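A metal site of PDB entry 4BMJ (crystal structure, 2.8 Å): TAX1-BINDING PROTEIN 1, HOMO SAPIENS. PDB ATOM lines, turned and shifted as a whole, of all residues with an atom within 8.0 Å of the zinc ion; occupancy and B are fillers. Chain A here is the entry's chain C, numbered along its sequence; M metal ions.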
ATOM      1  N   VAL A  36     -24.222  14.918   4.523  1.00  0.00           N
ATOM      2  CA  VAL A  36     -25.641  14.577   4.461  1.00  0.00           C
ATOM      3  C   VAL A  36     -26.169  14.407   3.033  1.00  0.00           C
ATOM      4  O   VAL A  36     -25.817  15.158   2.152  1.00  0.00           O
ATOM      5  CB  VAL A  36     -26.463  15.640   5.125  1.00  0.00           C
ATOM      6  CG1 VAL A  36     -27.935  15.290   5.018  1.00  0.00           C
ATOM      7  CG2 VAL A  36     -26.040  15.800   6.557  1.00  0.00           C
ATOM      8  N   CYS A  37     -27.034  13.428   2.820  1.00  0.00           N
ATOM      9  CA  CYS A  37     -27.624  13.262   1.498  1.00  0.00           C
ATOM     10  C   CYS A  37     -28.856  14.128   1.274  1.00  0.00           C
ATOM     11  O   CYS A  37     -29.856  14.003   1.983  1.00  0.00           O
ATOM     12  CB  CYS A  37     -28.011  11.801   1.292  1.00  0.00           C
ATOM     13  SG  CYS A  37     -28.807  11.602  -0.285  1.00  0.00           S
ATOM     14  N   PRO A  38     -28.825  14.983   0.252  1.00  0.00           N
ATOM     15  CA  PRO A  38     -29.930  15.900  -0.018  1.00  0.00           C
ATOM     16  C   PRO A  38     -31.248  15.183  -0.359  1.00  0.00           C
ATOM     17  O   PRO A  38     -32.338  15.740  -0.152  1.00  0.00           O
ATOM     18  CB  PRO A  38     -29.435  16.706  -1.229  1.00  0.00           C
ATOM     19  CG  PRO A  38     -27.964  16.415  -1.343  1.00  0.00           C
ATOM     20  CD  PRO A  38     -27.765  15.067  -0.759  1.00  0.00           C
ATOM     21  N   MET A  39     -31.170  13.970  -0.880  1.00  0.00           N
ATOM     22  CA  MET A  39     -32.391  13.242  -1.188  1.00  0.00           C
ATOM     23  C   MET A  39     -33.001  12.567   0.043  1.00  0.00           C
ATOM     24  O   MET A  39     -34.204  12.671   0.284  1.00  0.00           O
ATOM     25  CB  MET A  39     -32.156  12.218  -2.296  1.00  0.00           C
ATOM     26  CG  MET A  39     -31.618  12.839  -3.580  1.00  0.00           C
ATOM     27  SD  MET A  39     -32.777  14.037  -4.264  1.00  0.00           S
ATOM     28  CE  MET A  39     -33.422  13.116  -5.643  1.00  0.00           C
ATOM     29  N   CYS A  40     -32.163  11.918   0.859  1.00  0.00           N
ATOM     30  CA  CYS A  40     -32.682  11.030   1.904  1.00  0.00           C
ATOM     31  C   CYS A  40     -32.171  11.307   3.309  1.00  0.00           C
ATOM     32  O   CYS A  40     -32.655  10.685   4.249  1.00  0.00           O
ATOM     33  CB  CYS A  40     -32.405   9.563   1.556  1.00  0.00           C
ATOM     34  SG  CYS A  40     -30.650   9.187   1.373  1.00  0.00           S
ATOM     35  N   SER A  41     -31.190  12.197   3.467  1.00  0.00           N
ATOM     36  CA  SER A  41     -30.637  12.478   4.800  1.00  0.00           C
ATOM     37  C   SER A  41     -29.758  11.394   5.404  1.00  0.00           C
ATOM     38  O   SER A  41     -29.306  11.544   6.540  1.00  0.00           O
ATOM     39  CB  SER A  41     -31.747  12.772   5.798  1.00  0.00           C
ATOM     40  OG  SER A  41     -32.625  13.711   5.238  1.00  0.00           O
ATOM     41  N   GLU A  42     -29.528  10.289   4.699  1.00  0.00           N
ATOM     42  CA  GLU A  42     -28.404   9.461   5.089  1.00  0.00           C
ATOM     43  C   GLU A  42     -27.238  10.378   5.485  1.00  0.00           C
ATOM     44  O   GLU A  42     -26.959  11.388   4.798  1.00  0.00           O
ATOM     45  CB  GLU A  42     -27.944   8.626   3.938  1.00  0.00           C
ATOM     46  CG  GLU A  42     -26.858   7.687   4.357  1.00  0.00           C
ATOM     47  CD  GLU A  42     -27.348   6.713   5.418  1.00  0.00           C
ATOM     48  OE1 GLU A  42     -28.289   5.959   5.106  1.00  0.00           O
ATOM     49  OE2 GLU A  42     -26.821   6.724   6.554  1.00  0.00           O
ATOM     50  N   GLN A  43     -26.565  10.075   6.571  1.00  0.00           N
ATOM     51  CA  GLN A  43     -25.440  10.899   6.990  1.00  0.00           C
ATOM     52  C   GLN A  43     -24.207  10.031   6.918  1.00  0.00           C
ATOM     53  O   GLN A  43     -24.316   8.815   6.988  1.00  0.00           O
ATOM     54  CB  GLN A  43     -25.652  11.420   8.410  1.00  0.00           C
ATOM     55  CG  GLN A  43     -27.104  11.776   8.703  1.00  0.00           C
ATOM     56  CD  GLN A  43     -27.256  12.632   9.959  1.00  0.00           C
ATOM     57  OE1 GLN A  43     -26.970  13.843   9.952  1.00  0.00           O
ATOM     58  NE2 GLN A  43     -27.727  12.008  11.032  1.00  0.00           N
ATOM     59  N   PHE A  44     -23.042  10.641   6.769  1.00  0.00           N
ATOM     60  CA  PHE A  44     -21.786   9.883   6.641  1.00  0.00           C
ATOM     61  C   PHE A  44     -20.674  10.574   7.426  1.00  0.00           C
ATOM     62  O   PHE A  44     -20.768  11.759   7.750  1.00  0.00           O
ATOM     63  CB  PHE A  44     -21.354   9.755   5.160  1.00  0.00           C
ATOM     64  CG  PHE A  44     -22.462   9.359   4.197  1.00  0.00           C
ATOM     65  CD1 PHE A  44     -23.532  10.198   3.933  1.00  0.00           C
ATOM     66  CD2 PHE A  44     -22.387   8.145   3.499  1.00  0.00           C
ATOM     67  CE1 PHE A  44     -24.544   9.817   3.025  1.00  0.00           C
ATOM     68  CE2 PHE A  44     -23.391   7.767   2.596  1.00  0.00           C
ATOM     69  CZ  PHE A  44     -24.472   8.594   2.366  1.00  0.00           C
ATOM     70  N   PHE A  53     -19.640   8.846  -1.854  1.00  0.00           N
ATOM     71  CA  PHE A  53     -20.760   9.653  -1.387  1.00  0.00           C
ATOM     72  C   PHE A  53     -21.598  10.120  -2.571  1.00  0.00           C
ATOM     73  O   PHE A  53     -22.795   9.865  -2.630  1.00  0.00           O
ATOM     74  CB  PHE A  53     -20.304  10.844  -0.594  1.00  0.00           C
ATOM     75  CG  PHE A  53     -21.411  11.809  -0.309  1.00  0.00           C
ATOM     76  CD1 PHE A  53     -22.213  11.657   0.808  1.00  0.00           C
ATOM     77  CD2 PHE A  53     -21.664  12.872  -1.166  1.00  0.00           C
ATOM     78  CE1 PHE A  53     -23.238  12.564   1.083  1.00  0.00           C
ATOM     79  CE2 PHE A  53     -22.690  13.775  -0.905  1.00  0.00           C
ATOM     80  CZ  PHE A  53     -23.491  13.613   0.215  1.00  0.00           C
ATOM     81  N   ARG A  55     -21.886   8.936  -5.361  1.00  0.00           N
ATOM     82  CA  ARG A  55     -22.532   7.838  -6.058  1.00  0.00           C
ATOM     83  C   ARG A  55     -23.820   7.501  -5.331  1.00  0.00           C
ATOM     84  O   ARG A  55     -24.813   7.132  -5.955  1.00  0.00           O
ATOM     85  CB  ARG A  55     -21.624   6.611  -6.168  1.00  0.00           C
ATOM     86  CG  ARG A  55     -22.266   5.434  -6.886  1.00  0.00           C
ATOM     87  CD  ARG A  55     -21.193   4.537  -7.389  1.00  0.00           C
ATOM     88  NE  ARG A  55     -20.017   4.725  -6.553  1.00  0.00           N
ATOM     89  CZ  ARG A  55     -18.771   4.582  -6.976  1.00  0.00           C
ATOM     90  NH1 ARG A  55     -18.549   4.239  -8.222  1.00  0.00           N
ATOM     91  NH2 ARG A  55     -17.760   4.785  -6.140  1.00  0.00           N
ATOM     92  N   HIS A  56     -23.806   7.648  -4.014  1.00  0.00           N
ATOM     93  CA  HIS A  56     -25.017   7.382  -3.248  1.00  0.00           C
ATOM     94  C   HIS A  56     -26.110   8.319  -3.740  1.00  0.00           C
ATOM     95  O   HIS A  56     -27.150   7.890  -4.232  1.00  0.00           O
ATOM     96  CB  HIS A  56     -24.796   7.564  -1.742  1.00  0.00           C
ATOM     97  CG  HIS A  56     -26.073   7.689  -0.977  1.00  0.00           C
ATOM     98  ND1 HIS A  56     -26.690   6.623  -0.361  1.00  0.00           N
ATOM     99  CD2 HIS A  56     -26.897   8.759  -0.789  1.00  0.00           C
ATOM    100  CE1 HIS A  56     -27.806   7.031   0.204  1.00  0.00           C
ATOM    101  NE2 HIS A  56     -27.955   8.326  -0.042  1.00  0.00           N
ATOM    102  N   VAL A  57     -25.848   9.612  -3.637  1.00  0.00           N
ATOM    103  CA  VAL A  57     -26.794  10.622  -4.110  1.00  0.00           C
ATOM    104  C   VAL A  57     -27.306  10.342  -5.529  1.00  0.00           C
ATOM    105  O   VAL A  57     -28.514  10.296  -5.761  1.00  0.00           O
ATOM    106  CB  VAL A  57     -26.182  12.020  -4.057  1.00  0.00           C
ATOM    107  CG1 VAL A  57     -27.063  12.997  -4.776  1.00  0.00           C
ATOM    108  CG2 VAL A  57     -25.963  12.449  -2.603  1.00  0.00           C
ATOM    109  N   GLN A  58     -26.378  10.102  -6.456  1.00  0.00           N
ATOM    110  CA  GLN A  58     -26.752   9.906  -7.850  1.00  0.00           C
ATOM    111  C   GLN A  58     -27.742   8.764  -8.005  1.00  0.00           C
ATOM    112  O   GLN A  58     -28.625   8.806  -8.872  1.00  0.00           O
ATOM    113  CB  GLN A  58     -25.530   9.673  -8.749  1.00  0.00           C
ATOM    114  CG  GLN A  58     -25.865   9.718 -10.226  1.00  0.00           C
ATOM    115  CD  GLN A  58     -26.399  11.075 -10.662  1.00  0.00           C
ATOM    116  OE1 GLN A  58     -26.310  12.056  -9.920  1.00  0.00           O
ATOM    117  NE2 GLN A  58     -26.973  11.133 -11.867  1.00  0.00           N
ATOM    118  N   THR A  59     -27.608   7.732  -7.179  1.00  0.00           N
ATOM    119  CA  THR A  59     -28.438   6.559  -7.388  1.00  0.00           C
ATOM    120  C   THR A  59     -29.922   6.838  -7.203  1.00  0.00           C
ATOM    121  O   THR A  59     -30.756   6.255  -7.900  1.00  0.00           O
ATOM    122  CB  THR A  59     -28.005   5.431  -6.495  1.00  0.00           C
ATOM    123  OG1 THR A  59     -26.688   5.056  -6.876  1.00  0.00           O
ATOM    124  CG2 THR A  59     -28.919   4.252  -6.696  1.00  0.00           C
ATOM    125  N   HIS A  60     -30.240   7.711  -6.258  1.00  0.00           N
ATOM    126  CA  HIS A  60     -31.591   8.164  -6.098  1.00  0.00           C
ATOM    127  C   HIS A  60     -32.165   8.555  -7.492  1.00  0.00           C
ATOM    128  O   HIS A  60     -33.336   8.303  -7.798  1.00  0.00           O
ATOM    129  CB  HIS A  60     -31.632   9.354  -5.135  1.00  0.00           C
ATOM    130  CG  HIS A  60     -31.330   9.018  -3.709  1.00  0.00           C
ATOM    131  ND1 HIS A  60     -32.230   8.385  -2.876  1.00  0.00           N
ATOM    132  CD2 HIS A  60     -30.245   9.295  -2.930  1.00  0.00           C
ATOM    133  CE1 HIS A  60     -31.700   8.259  -1.670  1.00  0.00           C
ATOM    134  NE2 HIS A  60     -30.503   8.811  -1.670  1.00  0.00           N
HETATM  135 ZN    ZN M   1     -29.459   9.437  -0.083  1.00  0.00          ZN
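O of Glu 42 is in hydrogen-bond range of N of Cys 37. The side-chain sulfur of Cys 40 lies close to the backbone NH of Glu 42 (3.7 Å). SG of Cys 37 lies close to N of Met 39, at 3.4 Å.
The zinc ion is bound by NE2 of His 56, SG of Cys 40, NE2 of His 60 and SG of Cys 37.
Of the 16 residues printed, 4 come within 4 Å of the zinc ion. The nearest printed residue that does not touch the zinc ion is Glu 42 (4.4 Å).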
